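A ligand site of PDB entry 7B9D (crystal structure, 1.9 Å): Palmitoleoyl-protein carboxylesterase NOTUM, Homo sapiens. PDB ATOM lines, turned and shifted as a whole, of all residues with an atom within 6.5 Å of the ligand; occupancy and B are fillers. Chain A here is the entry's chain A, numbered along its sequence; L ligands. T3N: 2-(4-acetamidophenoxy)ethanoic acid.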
ATOM      1  N   GLY A  49      -5.416  -4.422  19.835  1.00  0.00           N
ATOM      2  CA  GLY A  49      -6.352  -3.358  20.090  1.00  0.00           C
ATOM      3  C   GLY A  49      -5.916  -2.028  19.485  1.00  0.00           C
ATOM      4  O   GLY A  49      -4.960  -1.943  18.715  1.00  0.00           O
ATOM      5  N   GLY A  50      -6.678  -0.972  19.834  1.00  0.00           N
ATOM      6  CA  GLY A  50      -6.391   0.382  19.368  1.00  0.00           C
ATOM      7  C   GLY A  50      -7.567   1.268  18.948  1.00  0.00           C
ATOM      8  O   GLY A  50      -7.503   1.899  17.882  1.00  0.00           O
ATOM      9  N   TRP A  51      -8.613   1.338  19.759  1.00  0.00           N
ATOM     10  CA  TRP A  51      -9.828   2.191  19.567  1.00  0.00           C
ATOM     11  C   TRP A  51     -10.487   1.822  18.225  1.00  0.00           C
ATOM     12  O   TRP A  51     -10.575   0.631  17.904  1.00  0.00           O
ATOM     13  CB  TRP A  51      -9.460   3.685  19.724  1.00  0.00           C
ATOM     14  CG  TRP A  51      -9.123   4.070  21.150  1.00  0.00           C
ATOM     15  CD1 TRP A  51      -7.882   4.152  21.700  1.00  0.00           C
ATOM     16  CD2 TRP A  51     -10.048   4.406  22.195  1.00  0.00           C
ATOM     17  NE1 TRP A  51      -7.975   4.522  23.017  1.00  0.00           N
ATOM     18  CE2 TRP A  51      -9.288   4.686  23.346  1.00  0.00           C
ATOM     19  CE3 TRP A  51     -11.441   4.506  22.253  1.00  0.00           C
ATOM     20  CZ2 TRP A  51      -9.878   5.051  24.562  1.00  0.00           C
ATOM     21  CZ3 TRP A  51     -12.019   4.869  23.463  1.00  0.00           C
ATOM     22  CH2 TRP A  51     -11.243   5.145  24.598  1.00  0.00           C
ATOM     23  N   TYR A  52     -10.991   2.809  17.461  1.00  0.00           N
ATOM     24  CA  TYR A  52     -11.741   2.626  16.218  1.00  0.00           C
ATOM     25  C   TYR A  52     -12.009   4.010  15.610  1.00  0.00           C
ATOM     26  O   TYR A  52     -11.700   5.036  16.211  1.00  0.00           O
ATOM     27  CB  TYR A  52     -13.071   1.885  16.436  1.00  0.00           C
ATOM     28  CG  TYR A  52     -13.987   2.547  17.439  1.00  0.00           C
ATOM     29  CD1 TYR A  52     -14.985   3.426  17.026  1.00  0.00           C
ATOM     30  CD2 TYR A  52     -13.878   2.277  18.793  1.00  0.00           C
ATOM     31  CE1 TYR A  52     -15.836   4.032  17.947  1.00  0.00           C
ATOM     32  CE2 TYR A  52     -14.731   2.877  19.726  1.00  0.00           C
ATOM     33  CZ  TYR A  52     -15.701   3.751  19.291  1.00  0.00           C
ATOM     34  OH  TYR A  52     -16.539   4.347  20.208  1.00  0.00           O
ATOM     35  N   TYR A 105      -4.310  -5.252  14.018  1.00  0.00           N
ATOM     36  CA  TYR A 105      -5.596  -4.557  13.906  1.00  0.00           C
ATOM     37  C   TYR A 105      -5.452  -3.474  12.848  1.00  0.00           C
ATOM     38  O   TYR A 105      -4.840  -2.432  13.085  1.00  0.00           O
ATOM     39  CB  TYR A 105      -5.978  -3.990  15.273  1.00  0.00           C
ATOM     40  CG  TYR A 105      -7.294  -3.252  15.423  1.00  0.00           C
ATOM     41  CD1 TYR A 105      -8.471  -3.711  14.836  1.00  0.00           C
ATOM     42  CD2 TYR A 105      -7.377  -2.140  16.238  1.00  0.00           C
ATOM     43  CE1 TYR A 105      -9.693  -3.028  15.023  1.00  0.00           C
ATOM     44  CE2 TYR A 105      -8.570  -1.470  16.441  1.00  0.00           C
ATOM     45  CZ  TYR A 105      -9.723  -1.913  15.834  1.00  0.00           C
ATOM     46  OH  TYR A 105     -10.897  -1.231  16.039  1.00  0.00           O
ATOM     47  N   VAL A 110     -13.477  -2.517  15.682  1.00  0.00           N
ATOM     48  CA  VAL A 110     -13.576  -3.351  16.876  1.00  0.00           C
ATOM     49  C   VAL A 110     -13.771  -4.815  16.427  1.00  0.00           C
ATOM     50  O   VAL A 110     -14.411  -5.625  17.111  1.00  0.00           O
ATOM     51  CB  VAL A 110     -14.725  -2.841  17.792  1.00  0.00           C
ATOM     52  CG1 VAL A 110     -14.826  -3.642  19.085  1.00  0.00           C
ATOM     53  CG2 VAL A 110     -14.644  -1.297  18.001  1.00  0.00           C
ATOM     54  N   SER A 154      -6.811  -7.857  23.388  1.00  0.00           N
ATOM     55  CA  SER A 154      -6.678  -6.810  24.407  1.00  0.00           C
ATOM     56  C   SER A 154      -7.358  -5.507  23.959  1.00  0.00           C
ATOM     57  O   SER A 154      -7.201  -5.090  22.804  1.00  0.00           O
ATOM     58  CB  SER A 154      -5.195  -6.496  24.746  1.00  0.00           C
ATOM     59  OG  SER A 154      -4.490  -7.577  25.343  1.00  0.00           O
ATOM     60  N   SER A 155      -8.080  -4.876  24.894  1.00  0.00           N
ATOM     61  CA  SER A 155      -8.802  -3.603  24.683  1.00  0.00           C
ATOM     62  C   SER A 155      -9.817  -3.797  23.562  1.00  0.00           C
ATOM     63  O   SER A 155     -10.728  -4.620  23.728  1.00  0.00           O
ATOM     64  CB  SER A 155      -7.808  -2.460  24.446  1.00  0.00           C
ATOM     65  OG  SER A 155      -6.652  -2.600  25.234  1.00  0.00           O
ATOM     66  N   ALA A 156      -9.724  -3.056  22.440  1.00  0.00           N
ATOM     67  CA  ALA A 156     -10.654  -3.280  21.335  1.00  0.00           C
ATOM     68  C   ALA A 156     -10.552  -4.712  20.823  1.00  0.00           C
ATOM     69  O   ALA A 156     -11.534  -5.260  20.308  1.00  0.00           O
ATOM     70  CB  ALA A 156     -10.387  -2.289  20.194  1.00  0.00           C
ATOM     71  N   GLY A 157      -9.374  -5.337  20.977  1.00  0.00           N
ATOM     72  CA  GLY A 157      -9.236  -6.745  20.656  1.00  0.00           C
ATOM     73  C   GLY A 157      -9.942  -7.636  21.651  1.00  0.00           C
ATOM     74  O   GLY A 157     -10.419  -8.709  21.293  1.00  0.00           O
ATOM     75  N   THR A 159     -12.853  -6.846  23.213  1.00  0.00           N
ATOM     76  CA  THR A 159     -14.237  -6.828  22.738  1.00  0.00           C
ATOM     77  C   THR A 159     -14.387  -7.699  21.493  1.00  0.00           C
ATOM     78  O   THR A 159     -15.413  -8.363  21.307  1.00  0.00           O
ATOM     79  CB  THR A 159     -14.690  -5.394  22.415  1.00  0.00           C
ATOM     80  OG1 THR A 159     -14.436  -4.530  23.521  1.00  0.00           O
ATOM     81  CG2 THR A 159     -16.198  -5.324  22.123  1.00  0.00           C
ATOM     82  N   SER A 188      -9.295  -6.595  29.054  1.00  0.00           N
ATOM     83  CA  SER A 188      -9.571  -5.143  29.060  1.00  0.00           C
ATOM     84  C   SER A 188     -10.603  -4.723  28.007  1.00  0.00           C
ATOM     85  O   SER A 188     -10.566  -3.596  27.516  1.00  0.00           O
ATOM     86  CB  SER A 188      -8.299  -4.319  28.884  1.00  0.00           C
ATOM     87  OG  SER A 188      -7.422  -4.459  29.985  1.00  0.00           O
ATOM     88  N   PHE A 191     -16.565  -3.232  28.999  1.00  0.00           N
ATOM     89  CA  PHE A 191     -16.946  -1.857  29.302  1.00  0.00           C
ATOM     90  C   PHE A 191     -18.405  -1.725  29.756  1.00  0.00           C
ATOM     91  O   PHE A 191     -19.252  -2.598  29.508  1.00  0.00           O
ATOM     92  CB  PHE A 191     -16.724  -0.923  28.097  1.00  0.00           C
ATOM     93  CG  PHE A 191     -15.335  -1.005  27.493  1.00  0.00           C
ATOM     94  CD1 PHE A 191     -15.086  -1.764  26.371  1.00  0.00           C
ATOM     95  CD2 PHE A 191     -14.270  -0.320  28.083  1.00  0.00           C
ATOM     96  CE1 PHE A 191     -13.807  -1.837  25.816  1.00  0.00           C
ATOM     97  CE2 PHE A 191     -12.985  -0.399  27.542  1.00  0.00           C
ATOM     98  CZ  PHE A 191     -12.761  -1.165  26.403  1.00  0.00           C
ATOM     99  N   LEU A 192     -18.680  -0.611  30.429  1.00  0.00           N
ATOM    100  CA  LEU A 192     -19.999  -0.272  30.933  1.00  0.00           C
ATOM    101  C   LEU A 192     -20.544   0.920  30.158  1.00  0.00           C
ATOM    102  O   LEU A 192     -19.803   1.874  29.883  1.00  0.00           O
ATOM    103  CB  LEU A 192     -19.940   0.084  32.428  1.00  0.00           C
ATOM    104  CG  LEU A 192     -19.386  -1.009  33.373  1.00  0.00           C
ATOM    105  CD1 LEU A 192     -19.457  -0.578  34.833  1.00  0.00           C
ATOM    106  CD2 LEU A 192     -20.093  -2.345  33.162  1.00  0.00           C
ATOM    107  N   PRO A 210     -20.299   7.664  23.693  1.00  0.00           N
ATOM    108  CA  PRO A 210     -19.749   6.442  23.114  1.00  0.00           C
ATOM    109  C   PRO A 210     -20.791   5.495  22.525  1.00  0.00           C
ATOM    110  O   PRO A 210     -20.528   4.944  21.454  1.00  0.00           O
ATOM    111  CB  PRO A 210     -19.034   5.793  24.306  1.00  0.00           C
ATOM    112  CG  PRO A 210     -18.542   6.960  25.069  1.00  0.00           C
ATOM    113  CD  PRO A 210     -19.592   8.036  24.940  1.00  0.00           C
ATOM    114  N   THR A 211     -21.940   5.306  23.184  1.00  0.00           N
ATOM    115  CA  THR A 211     -22.955   4.437  22.603  1.00  0.00           C
ATOM    116  C   THR A 211     -23.371   4.941  21.227  1.00  0.00           C
ATOM    117  O   THR A 211     -23.595   4.152  20.306  1.00  0.00           O
ATOM    118  CB  THR A 211     -24.184   4.321  23.499  1.00  0.00           C
ATOM    119  OG1 THR A 211     -24.712   5.613  23.777  1.00  0.00           O
ATOM    120  CG2 THR A 211     -23.832   3.639  24.798  1.00  0.00           C
ATOM    121  N   ALA A 213     -21.461   6.685  19.177  1.00  0.00           N
ATOM    122  CA  ALA A 213     -20.361   6.423  18.256  1.00  0.00           C
ATOM    123  C   ALA A 213     -20.368   4.971  17.768  1.00  0.00           C
ATOM    124  O   ALA A 213     -20.152   4.715  16.578  1.00  0.00           O
ATOM    125  CB  ALA A 213     -19.029   6.762  18.922  1.00  0.00           C
ATOM    126  N   ILE A 214     -20.638   4.019  18.676  1.00  0.00           N
ATOM    127  CA  ILE A 214     -20.740   2.609  18.275  1.00  0.00           C
ATOM    128  C   ILE A 214     -21.906   2.406  17.315  1.00  0.00           C
ATOM    129  O   ILE A 214     -21.761   1.734  16.285  1.00  0.00           O
ATOM    130  CB  ILE A 214     -20.862   1.705  19.516  1.00  0.00           C
ATOM    131  CG1 ILE A 214     -19.587   1.780  20.355  1.00  0.00           C
ATOM    132  CG2 ILE A 214     -21.114   0.261  19.108  1.00  0.00           C
ATOM    133  CD1 ILE A 214     -18.402   1.161  19.672  1.00  0.00           C
ATOM    134  N   PHE A 242     -21.945  -4.902  21.923  1.00  0.00           N
ATOM    135  CA  PHE A 242     -20.559  -4.496  22.147  1.00  0.00           C
ATOM    136  C   PHE A 242     -20.236  -4.315  23.631  1.00  0.00           C
ATOM    137  O   PHE A 242     -19.091  -3.976  23.959  1.00  0.00           O
ATOM    138  CB  PHE A 242     -20.218  -3.167  21.433  1.00  0.00           C
ATOM    139  CG  PHE A 242     -20.050  -3.288  19.931  1.00  0.00           C
ATOM    140  CD1 PHE A 242     -21.072  -3.799  19.126  1.00  0.00           C
ATOM    141  CD2 PHE A 242     -18.855  -2.908  19.327  1.00  0.00           C
ATOM    142  CE1 PHE A 242     -20.910  -3.918  17.754  1.00  0.00           C
ATOM    143  CE2 PHE A 242     -18.680  -3.038  17.952  1.00  0.00           C
ATOM    144  CZ  PHE A 242     -19.717  -3.545  17.163  1.00  0.00           C
ATOM    145  N   PHE A 243     -21.197  -4.518  24.524  1.00  0.00           N
ATOM    146  CA  PHE A 243     -20.967  -4.401  25.963  1.00  0.00           C
ATOM    147  C   PHE A 243     -20.948  -5.793  26.600  1.00  0.00           C
ATOM    148  O   PHE A 243     -21.951  -6.516  26.549  1.00  0.00           O
ATOM    149  CB  PHE A 243     -21.993  -3.484  26.618  1.00  0.00           C
ATOM    150  CG  PHE A 243     -21.840  -2.048  26.203  1.00  0.00           C
ATOM    151  CD1 PHE A 243     -22.321  -1.604  24.977  1.00  0.00           C
ATOM    152  CD2 PHE A 243     -21.115  -1.166  26.979  1.00  0.00           C
ATOM    153  CE1 PHE A 243     -22.128  -0.299  24.572  1.00  0.00           C
ATOM    154  CE2 PHE A 243     -20.907   0.144  26.555  1.00  0.00           C
ATOM    155  CZ  PHE A 243     -21.423   0.564  25.359  1.00  0.00           C
ATOM    156  N   ALA A 265      -9.313   3.181  29.659  1.00  0.00           N
ATOM    157  CA  ALA A 265     -10.197   3.525  28.537  1.00  0.00           C
ATOM    158  C   ALA A 265     -11.613   3.796  29.018  1.00  0.00           C
ATOM    159  O   ALA A 265     -12.310   4.665  28.479  1.00  0.00           O
ATOM    160  CB  ALA A 265     -10.183   2.414  27.489  1.00  0.00           C
ATOM    161  N   VAL A 269     -13.731   7.351  28.375  1.00  0.00           N
ATOM    162  CA  VAL A 269     -15.073   7.541  27.838  1.00  0.00           C
ATOM    163  C   VAL A 269     -16.042   8.056  28.890  1.00  0.00           C
ATOM    164  O   VAL A 269     -17.132   8.514  28.532  1.00  0.00           O
ATOM    165  CB  VAL A 269     -15.640   6.257  27.185  1.00  0.00           C
ATOM    166  CG1 VAL A 269     -14.732   5.770  26.071  1.00  0.00           C
ATOM    167  CG2 VAL A 269     -15.872   5.162  28.227  1.00  0.00           C
ATOM    168  N   HIS A 312      -4.239  -0.453  31.903  1.00  0.00           N
ATOM    169  CA  HIS A 312      -4.781  -0.716  30.568  1.00  0.00           C
ATOM    170  C   HIS A 312      -4.014  -1.877  29.934  1.00  0.00           C
ATOM    171  O   HIS A 312      -2.795  -1.779  29.778  1.00  0.00           O
ATOM    172  CB  HIS A 312      -4.680   0.546  29.705  1.00  0.00           C
ATOM    173  CG  HIS A 312      -5.246   0.391  28.317  1.00  0.00           C
ATOM    174  ND1 HIS A 312      -6.581   0.143  28.084  1.00  0.00           N
ATOM    175  CD2 HIS A 312      -4.648   0.473  27.108  1.00  0.00           C
ATOM    176  CE1 HIS A 312      -6.785   0.074  26.781  1.00  0.00           C
ATOM    177  NE2 HIS A 312      -5.630   0.277  26.164  1.00  0.00           N
ATOM    178  N   GLU A 313      -4.721  -2.955  29.577  1.00  0.00           N
ATOM    179  CA  GLU A 313      -4.173  -4.193  29.013  1.00  0.00           C
ATOM    180  C   GLU A 313      -3.272  -4.927  30.009  1.00  0.00           C
ATOM    181  O   GLU A 313      -2.797  -4.318  30.972  1.00  0.00           O
ATOM    182  CB  GLU A 313      -3.388  -3.947  27.717  1.00  0.00           C
ATOM    183  CG  GLU A 313      -4.205  -3.294  26.621  1.00  0.00           C
ATOM    184  CD  GLU A 313      -3.447  -3.071  25.324  1.00  0.00           C
ATOM    185  OE1 GLU A 313      -4.056  -2.616  24.316  1.00  0.00           O
ATOM    186  OE2 GLU A 313      -2.225  -3.358  25.310  1.00  0.00           O
HETATM  187  C10 T3N L   1     -14.007   1.550  23.916  1.00  0.00           C
HETATM  188  C13 T3N L   1      -8.524   0.456  23.079  1.00  0.00           C
HETATM  189  C01 T3N L   1     -18.557   2.114  23.760  1.00  0.00           C
HETATM  190  C02 T3N L   1     -17.049   2.104  23.471  1.00  0.00           C
HETATM  191  C05 T3N L   1     -14.891   0.752  23.203  1.00  0.00           C
HETATM  192  C06 T3N L   1     -14.419  -0.141  22.264  1.00  0.00           C
HETATM  193  C07 T3N L   1     -13.057  -0.232  22.017  1.00  0.00           C
HETATM  194  C08 T3N L   1     -12.171   0.573  22.718  1.00  0.00           C
HETATM  195  C09 T3N L   1     -12.637   1.470  23.669  1.00  0.00           C
HETATM  196  C12 T3N L   1      -9.937   0.884  23.490  1.00  0.00           C
HETATM  197  N04 T3N L   1     -16.328   0.841  23.458  1.00  0.00           N
HETATM  198  O03 T3N L   1     -16.498   3.140  23.260  1.00  0.00           O
HETATM  199  O11 T3N L   1     -10.794   0.477  22.456  1.00  0.00           O
HETATM  200  O14 T3N L   1      -7.521   0.875  23.708  1.00  0.00           O
HETATM  201  O15 T3N L   1      -8.365  -0.316  22.095  1.00  0.00           O
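Merely in contact with the ligand: Gly 49, Ser 155, Phe 191, Pro 210, Ile 214 and Phe 243. The nearest printed residue that does not touch the ligand is Val 269 (4.2 Å).
The side-chain hydroxyl (OG) of Ser 155 is in hydrogen-bond range of the side-chain carboxylate (OE1) of Glu 313 (2.8 Å). OH of Tyr 105 lies within hydrogen-bond range of O of Trp 51 (2.7 Å). A ring nitrogen (NE2) of His 312 sits close to the side-chain hydroxyl (OG) of Ser 155 (3.2 Å).
N of Ala 156 lies within hydrogen-bond range of O15 of the ligand (3.1 Å). OH of Tyr 52 sits at hydrogen-bond distance from O03 of the ligand, at 3.3 Å. O14 of the ligand sits at hydrogen-bond distance from NE2 of His 312 (3.2 Å). An oxygen (O15) of the ligand is in hydrogen-bond range of the backbone NH (N) of Gly 50 (2.9 Å). N of Trp 51 lies within hydrogen-bond range of O15 of the ligand (2.9 Å).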
